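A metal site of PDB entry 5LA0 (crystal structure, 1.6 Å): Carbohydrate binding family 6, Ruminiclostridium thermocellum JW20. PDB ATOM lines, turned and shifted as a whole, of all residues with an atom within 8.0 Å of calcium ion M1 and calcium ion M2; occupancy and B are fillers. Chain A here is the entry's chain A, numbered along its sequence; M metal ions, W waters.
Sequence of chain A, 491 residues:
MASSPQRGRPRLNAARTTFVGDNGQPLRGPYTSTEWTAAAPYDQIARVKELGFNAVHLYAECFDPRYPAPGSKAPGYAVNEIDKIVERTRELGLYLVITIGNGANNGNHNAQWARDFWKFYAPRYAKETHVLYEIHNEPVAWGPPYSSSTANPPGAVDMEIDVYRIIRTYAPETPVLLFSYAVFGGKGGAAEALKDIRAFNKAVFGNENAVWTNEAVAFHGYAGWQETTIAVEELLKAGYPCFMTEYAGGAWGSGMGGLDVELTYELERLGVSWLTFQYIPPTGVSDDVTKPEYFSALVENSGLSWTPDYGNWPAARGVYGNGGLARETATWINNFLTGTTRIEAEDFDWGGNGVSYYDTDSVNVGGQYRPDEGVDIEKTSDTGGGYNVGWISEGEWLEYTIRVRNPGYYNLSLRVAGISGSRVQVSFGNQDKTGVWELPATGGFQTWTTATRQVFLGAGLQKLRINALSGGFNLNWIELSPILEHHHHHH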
ATOM      1  N   ASN A 353       1.276 -23.474  25.872  1.00  0.00           N
ATOM      2  CA  ASN A 353       0.050 -24.094  25.470  1.00  0.00           C
ATOM      3  C   ASN A 353      -0.846 -24.257  26.686  1.00  0.00           C
ATOM      4  O   ASN A 353      -0.473 -24.857  27.711  1.00  0.00           O
ATOM      5  CB  ASN A 353       0.341 -25.440  24.814  1.00  0.00           C
ATOM      6  CG  ASN A 353      -0.637 -25.772  23.692  1.00  0.00           C
ATOM      7  OD1 ASN A 353      -1.747 -25.253  23.653  1.00  0.00           O
ATOM      8  ND2 ASN A 353      -0.222 -26.661  22.781  1.00  0.00           N
ATOM      9  N   TYR A 357      -1.627 -19.313  24.603  1.00  0.00           N
ATOM     10  CA  TYR A 357      -2.342 -19.775  23.420  1.00  0.00           C
ATOM     11  C   TYR A 357      -2.831 -21.184  23.717  1.00  0.00           C
ATOM     12  O   TYR A 357      -2.360 -21.809  24.674  1.00  0.00           O
ATOM     13  CB  TYR A 357      -1.420 -19.799  22.194  1.00  0.00           C
ATOM     14  CG  TYR A 357      -0.161 -20.652  22.340  1.00  0.00           C
ATOM     15  CD1 TYR A 357      -0.179 -22.037  22.075  1.00  0.00           C
ATOM     16  CD2 TYR A 357       1.029 -20.091  22.758  1.00  0.00           C
ATOM     17  CE1 TYR A 357       0.966 -22.808  22.194  1.00  0.00           C
ATOM     18  CE2 TYR A 357       2.175 -20.872  22.897  1.00  0.00           C
ATOM     19  CZ  TYR A 357       2.119 -22.231  22.608  1.00  0.00           C
ATOM     20  OH  TYR A 357       3.251 -23.017  22.749  1.00  0.00           O
ATOM     21  N   TYR A 358      -3.727 -21.688  22.902  1.00  0.00           N
ATOM     22  CA  TYR A 358      -4.076 -23.087  22.920  1.00  0.00           C
ATOM     23  C   TYR A 358      -3.996 -23.584  21.490  1.00  0.00           C
ATOM     24  O   TYR A 358      -4.642 -23.021  20.585  1.00  0.00           O
ATOM     25  CB  TYR A 358      -5.484 -23.344  23.495  1.00  0.00           C
ATOM     26  CG  TYR A 358      -5.862 -24.825  23.375  1.00  0.00           C
ATOM     27  CD1 TYR A 358      -5.280 -25.790  24.200  1.00  0.00           C
ATOM     28  CD2 TYR A 358      -6.745 -25.256  22.406  1.00  0.00           C
ATOM     29  CE1 TYR A 358      -5.590 -27.138  24.071  1.00  0.00           C
ATOM     30  CE2 TYR A 358      -7.067 -26.599  22.258  1.00  0.00           C
ATOM     31  CZ  TYR A 358      -6.489 -27.529  23.096  1.00  0.00           C
ATOM     32  OH  TYR A 358      -6.810 -28.850  22.959  1.00  0.00           O
ATOM     33  N   ASP A 359      -3.181 -24.631  21.296  1.00  0.00           N
ATOM     34  CA  ASP A 359      -3.002 -25.240  20.008  1.00  0.00           C
ATOM     35  C   ASP A 359      -3.172 -26.734  20.134  1.00  0.00           C
ATOM     36  O   ASP A 359      -2.644 -27.342  21.059  1.00  0.00           O
ATOM     37  CB  ASP A 359      -1.617 -24.953  19.417  1.00  0.00           C
ATOM     38  CG  ASP A 359      -1.639 -25.028  17.864  1.00  0.00           C
ATOM     39  OD1 ASP A 359      -1.989 -23.979  17.232  1.00  0.00           O
ATOM     40  OD2 ASP A 359      -1.401 -26.128  17.275  1.00  0.00           O
ATOM     41  N   THR A 360      -3.869 -27.323  19.168  1.00  0.00           N
ATOM     42  CA  THR A 360      -4.207 -28.748  19.184  1.00  0.00           C
ATOM     43  C   THR A 360      -2.971 -29.647  19.089  1.00  0.00           C
ATOM     44  O   THR A 360      -3.022 -30.780  19.568  1.00  0.00           O
ATOM     45  CB  THR A 360      -5.236 -29.100  18.081  1.00  0.00           C
ATOM     46  OG1 THR A 360      -4.701 -28.806  16.761  1.00  0.00           O
ATOM     47  CG2 THR A 360      -6.451 -28.271  18.272  1.00  0.00           C
ATOM     48  N   ASP A 361      -1.869 -29.170  18.494  1.00  0.00           N
ATOM     49  CA  ASP A 361      -0.600 -29.929  18.417  1.00  0.00           C
ATOM     50  C   ASP A 361       0.504 -29.069  19.011  1.00  0.00           C
ATOM     51  O   ASP A 361       0.591 -27.875  18.750  1.00  0.00           O
ATOM     52  CB  ASP A 361      -0.176 -30.326  16.978  1.00  0.00           C
ATOM     53  CG  ASP A 361      -1.340 -30.577  16.034  1.00  0.00           C
ATOM     54  OD1 ASP A 361      -2.322 -31.249  16.440  1.00  0.00           O
ATOM     55  OD2 ASP A 361      -1.258 -30.119  14.872  1.00  0.00           O
ATOM     56  N   SER A 362       1.368 -29.690  19.804  1.00  0.00           N
ATOM     57  CA  SER A 362       2.494 -29.004  20.399  1.00  0.00           C
ATOM     58  C   SER A 362       3.555 -28.498  19.405  1.00  0.00           C
ATOM     59  O   SER A 362       4.339 -27.643  19.742  1.00  0.00           O
ATOM     60  CB  SER A 362       3.157 -29.941  21.404  1.00  0.00           C
ATOM     61  OG  SER A 362       3.590 -31.129  20.767  1.00  0.00           O
ATOM     62  N   VAL A 363       3.603 -29.066  18.213  1.00  0.00           N
ATOM     63  CA  VAL A 363       4.534 -28.670  17.149  1.00  0.00           C
ATOM     64  C   VAL A 363       3.984 -27.498  16.353  1.00  0.00           C
ATOM     65  O   VAL A 363       2.774 -27.406  16.098  1.00  0.00           O
ATOM     66  CB  VAL A 363       4.834 -29.881  16.221  1.00  0.00           C
ATOM     67  CG1 VAL A 363       5.685 -29.479  15.018  1.00  0.00           C
ATOM     68  CG2 VAL A 363       5.556 -30.965  17.008  1.00  0.00           C
ATOM     69  N   ASN A 364       4.893 -26.606  15.976  1.00  0.00           N
ATOM     70  CA  ASN A 364       4.639 -25.541  15.002  1.00  0.00           C
ATOM     71  C   ASN A 364       4.919 -26.156  13.624  1.00  0.00           C
ATOM     72  O   ASN A 364       6.086 -26.223  13.187  1.00  0.00           O
ATOM     73  CB  ASN A 364       5.542 -24.348  15.284  1.00  0.00           C
ATOM     74  CG  ASN A 364       5.533 -23.300  14.173  1.00  0.00           C
ATOM     75  OD1 ASN A 364       4.873 -23.438  13.151  1.00  0.00           O
ATOM     76  ND2 ASN A 364       6.300 -22.236  14.396  1.00  0.00           N
ATOM     77  N   VAL A 365       3.854 -26.578  12.953  1.00  0.00           N
ATOM     78  CA  VAL A 365       4.046 -27.354  11.719  1.00  0.00           C
ATOM     79  C   VAL A 365       4.493 -26.531  10.561  1.00  0.00           C
ATOM     80  O   VAL A 365       5.035 -27.083   9.635  1.00  0.00           O
ATOM     81  CB  VAL A 365       2.852 -28.228  11.325  1.00  0.00           C
ATOM     82  CG1 VAL A 365       2.588 -29.256  12.415  1.00  0.00           C
ATOM     83  CG2 VAL A 365       1.607 -27.402  11.023  1.00  0.00           C
ATOM     84  N   GLY A 366       4.268 -25.226  10.614  1.00  0.00           N
ATOM     85  CA  GLY A 366       4.774 -24.290   9.610  1.00  0.00           C
ATOM     86  C   GLY A 366       6.278 -24.047   9.739  1.00  0.00           C
ATOM     87  O   GLY A 366       6.936 -23.746   8.752  1.00  0.00           O
ATOM     88  N   GLU A 373       7.503 -23.060  19.779  1.00  0.00           N
ATOM     89  CA  GLU A 373       6.181 -22.938  20.378  1.00  0.00           C
ATOM     90  C   GLU A 373       5.171 -23.678  19.527  1.00  0.00           C
ATOM     91  O   GLU A 373       5.497 -24.144  18.439  1.00  0.00           O
ATOM     92  CB  GLU A 373       5.869 -21.453  20.604  1.00  0.00           C
ATOM     93  CG  GLU A 373       6.650 -20.900  21.798  1.00  0.00           C
ATOM     94  CD  GLU A 373       6.793 -19.376  21.809  1.00  0.00           C
ATOM     95  OE1 GLU A 373       6.081 -18.756  22.615  1.00  0.00           O
ATOM     96  OE2 GLU A 373       7.628 -18.801  21.042  1.00  0.00           O
ATOM     97  N   GLY A 374       3.958 -23.826  20.048  1.00  0.00           N
ATOM     98  CA  GLY A 374       2.918 -24.702  19.474  1.00  0.00           C
ATOM     99  C   GLY A 374       2.048 -24.094  18.396  1.00  0.00           C
ATOM    100  O   GLY A 374       1.356 -24.825  17.670  1.00  0.00           O
ATOM    101  N   VAL A 375       2.090 -22.785  18.269  1.00  0.00           N
ATOM    102  CA  VAL A 375       1.321 -22.076  17.247  1.00  0.00           C
ATOM    103  C   VAL A 375       1.943 -22.328  15.867  1.00  0.00           C
ATOM    104  O   VAL A 375       3.150 -22.286  15.730  1.00  0.00           O
ATOM    105  CB  VAL A 375       1.190 -20.569  17.552  1.00  0.00           C
ATOM    106  CG1 VAL A 375       0.346 -19.862  16.493  1.00  0.00           C
ATOM    107  CG2 VAL A 375       0.529 -20.377  18.928  1.00  0.00           C
ATOM    108  N   ASP A 376       1.104 -22.550  14.865  1.00  0.00           N
ATOM    109  CA  ASP A 376       1.566 -22.903  13.522  1.00  0.00           C
ATOM    110  C   ASP A 376       1.701 -21.630  12.695  1.00  0.00           C
ATOM    111  O   ASP A 376       0.713 -20.900  12.506  1.00  0.00           O
ATOM    112  CB  ASP A 376       0.574 -23.879  12.915  1.00  0.00           C
ATOM    113  CG  ASP A 376       0.336 -25.070  13.823  1.00  0.00           C
ATOM    114  OD1 ASP A 376       1.330 -25.786  14.123  1.00  0.00           O
ATOM    115  OD2 ASP A 376      -0.795 -25.255  14.340  1.00  0.00           O
ATOM    116  N   ILE A 377       2.931 -21.354  12.245  1.00  0.00           N
ATOM    117  CA  ILE A 377       3.282 -20.100  11.602  1.00  0.00           C
ATOM    118  C   ILE A 377       4.039 -20.384  10.298  1.00  0.00           C
ATOM    119  O   ILE A 377       4.983 -21.163  10.260  1.00  0.00           O
ATOM    120  CB  ILE A 377       4.181 -19.209  12.508  1.00  0.00           C
ATOM    121  CG1 ILE A 377       3.576 -19.084  13.922  1.00  0.00           C
ATOM    122  CG2 ILE A 377       4.459 -17.847  11.861  1.00  0.00           C
ATOM    123  CD1 ILE A 377       4.481 -18.497  14.932  1.00  0.00           C
ATOM    124  N   VAL A 389      -0.310 -16.757  11.037  1.00  0.00           N
ATOM    125  CA  VAL A 389      -0.719 -17.926  11.763  1.00  0.00           C
ATOM    126  C   VAL A 389      -1.634 -18.723  10.842  1.00  0.00           C
ATOM    127  O   VAL A 389      -2.532 -18.166  10.196  1.00  0.00           O
ATOM    128  CB  VAL A 389      -1.444 -17.588  13.103  1.00  0.00           C
ATOM    129  CG1 VAL A 389      -2.007 -18.869  13.753  1.00  0.00           C
ATOM    130  CG2 VAL A 389      -0.507 -16.822  14.030  1.00  0.00           C
ATOM    131  N   GLY A 390      -1.379 -20.021  10.753  1.00  0.00           N
ATOM    132  CA  GLY A 390      -2.202 -20.939   9.955  1.00  0.00           C
ATOM    133  C   GLY A 390      -2.516 -22.191  10.733  1.00  0.00           C
ATOM    134  O   GLY A 390      -2.294 -22.253  11.972  1.00  0.00           O
ATOM    135  N   TRP A 391      -3.071 -23.177  10.047  1.00  0.00           N
ATOM    136  CA  TRP A 391      -3.463 -24.446  10.687  1.00  0.00           C
ATOM    137  C   TRP A 391      -4.313 -24.168  11.926  1.00  0.00           C
ATOM    138  O   TRP A 391      -4.060 -24.700  13.036  1.00  0.00           O
ATOM    139  CB  TRP A 391      -2.240 -25.305  11.012  1.00  0.00           C
ATOM    140  CG  TRP A 391      -1.393 -25.688   9.832  1.00  0.00           C
ATOM    141  CD1 TRP A 391      -1.470 -26.842   9.126  1.00  0.00           C
ATOM    142  CD2 TRP A 391      -0.355 -24.912   9.185  1.00  0.00           C
ATOM    143  NE1 TRP A 391      -0.562 -26.838   8.107  1.00  0.00           N
ATOM    144  CE2 TRP A 391       0.144 -25.671   8.119  1.00  0.00           C
ATOM    145  CE3 TRP A 391       0.205 -23.646   9.419  1.00  0.00           C
ATOM    146  CZ2 TRP A 391       1.178 -25.242   7.281  1.00  0.00           C
ATOM    147  CZ3 TRP A 391       1.236 -23.205   8.592  1.00  0.00           C
ATOM    148  CH2 TRP A 391       1.706 -24.028   7.531  1.00  0.00           C
ATOM    149  N   ILE A 392      -5.288 -23.289  11.749  1.00  0.00           N
ATOM    150  CA  ILE A 392      -6.144 -22.886  12.829  1.00  0.00           C
ATOM    151  C   ILE A 392      -7.329 -23.860  12.888  1.00  0.00           C
ATOM    152  O   ILE A 392      -7.963 -24.162  11.868  1.00  0.00           O
ATOM    153  CB  ILE A 392      -6.608 -21.432  12.686  1.00  0.00           C
ATOM    154  CG1 ILE A 392      -5.398 -20.517  12.549  1.00  0.00           C
ATOM    155  CG2 ILE A 392      -7.494 -21.064  13.873  1.00  0.00           C
ATOM    156  CD1 ILE A 392      -5.688 -19.033  12.548  1.00  0.00           C
ATOM    157  N   SER A 393      -7.618 -24.367  14.077  1.00  0.00           N
ATOM    158  CA  SER A 393      -8.760 -25.257  14.222  1.00  0.00           C
ATOM    159  C   SER A 393      -9.691 -24.840  15.347  1.00  0.00           C
ATOM    160  O   SER A 393      -9.326 -24.012  16.227  1.00  0.00           O
ATOM    161  CB  SER A 393      -8.285 -26.684  14.354  1.00  0.00           C
ATOM    162  OG  SER A 393      -7.776 -26.882  15.609  1.00  0.00           O
ATOM    163  N   GLU A 394     -10.887 -25.409  15.327  1.00  0.00           N
ATOM    164  CA  GLU A 394     -11.915 -25.045  16.305  1.00  0.00           C
ATOM    165  C   GLU A 394     -11.386 -25.199  17.730  1.00  0.00           C
ATOM    166  O   GLU A 394     -10.786 -26.201  18.044  1.00  0.00           O
ATOM    167  CB  GLU A 394     -13.156 -25.942  16.122  1.00  0.00           C
ATOM    168  CG  GLU A 394     -14.326 -25.522  16.986  1.00  0.00           C
ATOM    169  CD  GLU A 394     -15.556 -26.421  16.862  1.00  0.00           C
ATOM    170  OE1 GLU A 394     -15.686 -27.173  15.870  1.00  0.00           O
ATOM    171  OE2 GLU A 394     -16.418 -26.374  17.772  1.00  0.00           O
ATOM    172  N   GLU A 396      -8.961 -23.452  19.173  1.00  0.00           N
ATOM    173  CA  GLU A 396      -7.683 -22.781  19.324  1.00  0.00           C
ATOM    174  C   GLU A 396      -7.915 -21.331  19.758  1.00  0.00           C
ATOM    175  O   GLU A 396      -8.980 -20.745  19.509  1.00  0.00           O
ATOM    176  CB  GLU A 396      -6.808 -22.906  18.094  1.00  0.00           C
ATOM    177  CG  GLU A 396      -6.351 -24.334  17.853  1.00  0.00           C
ATOM    178  CD  GLU A 396      -5.218 -24.505  16.850  1.00  0.00           C
ATOM    179  OE1 GLU A 396      -5.039 -23.626  15.955  1.00  0.00           O
ATOM    180  OE2 GLU A 396      -4.517 -25.563  16.950  1.00  0.00           O
ATOM    181  N   TRP A 397      -6.933 -20.784  20.457  1.00  0.00           N
ATOM    182  CA  TRP A 397      -6.959 -19.374  20.833  1.00  0.00           C
ATOM    183  C   TRP A 397      -5.563 -18.797  21.010  1.00  0.00           C
ATOM    184  O   TRP A 397      -4.580 -19.530  21.118  1.00  0.00           O
ATOM    185  CB  TRP A 397      -7.840 -19.137  22.066  1.00  0.00           C
ATOM    186  CG  TRP A 397      -7.563 -19.990  23.296  1.00  0.00           C
ATOM    187  CD1 TRP A 397      -8.229 -21.109  23.674  1.00  0.00           C
ATOM    188  CD2 TRP A 397      -6.600 -19.732  24.337  1.00  0.00           C
ATOM    189  NE1 TRP A 397      -7.767 -21.573  24.900  1.00  0.00           N
ATOM    190  CE2 TRP A 397      -6.778 -20.726  25.331  1.00  0.00           C
ATOM    191  CE3 TRP A 397      -5.631 -18.736  24.552  1.00  0.00           C
ATOM    192  CZ2 TRP A 397      -5.986 -20.793  26.476  1.00  0.00           C
ATOM    193  CZ3 TRP A 397      -4.877 -18.764  25.695  1.00  0.00           C
ATOM    194  CH2 TRP A 397      -5.050 -19.805  26.656  1.00  0.00           C
ATOM    195  N   LEU A 398      -5.503 -17.481  20.961  1.00  0.00           N
ATOM    196  CA  LEU A 398      -4.282 -16.695  20.951  1.00  0.00           C
ATOM    197  C   LEU A 398      -4.499 -15.459  21.784  1.00  0.00           C
ATOM    198  O   LEU A 398      -5.525 -14.808  21.641  1.00  0.00           O
ATOM    199  CB  LEU A 398      -3.893 -16.265  19.539  1.00  0.00           C
ATOM    200  CG  LEU A 398      -3.762 -17.354  18.492  1.00  0.00           C
ATOM    201  CD1 LEU A 398      -3.945 -16.780  17.126  1.00  0.00           C
ATOM    202  CD2 LEU A 398      -2.393 -17.994  18.593  1.00  0.00           C
HETATM  203 CA    CA M   1       0.644 -26.684  16.360  1.00  0.00          CA
HETATM  204 CA    CA M   2      -2.936 -24.780  15.178  1.00  0.00          CA
HETATM  205  O   HOH W   1      -2.089 -22.492  14.633  1.00  0.00           O
HETATM  206  O   HOH W   2      -3.260 -27.142  14.802  1.00  0.00           O
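Water W1 bridges O of Gly 390 (2.7 Å) and N of Asp 376 (3.2 Å).
Four residues have an atom within 4 Å of calcium ion M2: Asp 359, Asp 376, Trp 391 and Glu 396.
Calcium ion M2 is bound by OD2 of Asp 376 (2.3 Å), OD1 of Asp 359 (2.4 Å), water W2 (2.4 Å), O of Trp 391 (2.4 Å), water W1 (2.5 Å), OE2 of Glu 396 (2.5 Å) and OE1 of Glu 396 (2.5 Å). Slightly farther from calcium ion M2 lies the side-chain carboxylate (OD2) of Asp 359 (2.9 Å).
Of the 25 residues printed, 5 come within 4 Å of calcium ion M1.
Calcium ion M1 is bound by O of Val 363 (2.3 Å), OD2 of Asp 359 (2.3 Å), O of Gly 374 (2.4 Å), OD1 of Asp 376 (2.5 Å), O of Asp 361 (2.7 Å) and OD2 of Asp 376 (2.9 Å).
The side-chain amide oxygen (OD1) of Asn 353 sits at hydrogen-bond distance from the backbone NH (N) of Asp 359 (2.8 Å). The backbone carbonyl oxygen of Asp 376 is in hydrogen-bond range of the backbone NH of Gly 390 (2.9 Å). The backbone NH (N) of Val 365 lies close to the side-chain carboxylate (OD1) of Asp 376. N of Gly 374 sits at hydrogen-bond distance from OH of Tyr 357 (2.9 Å). The side-chain carboxylate of Glu 396 sits close to the backbone NH of Thr 360. OE1 of Glu 396 sits close to N of Ser 393, at 3.3 Å. The side-chain hydroxyl of Thr 360 sits close to the side-chain carboxylate of Asp 361, 3.4 Å away.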
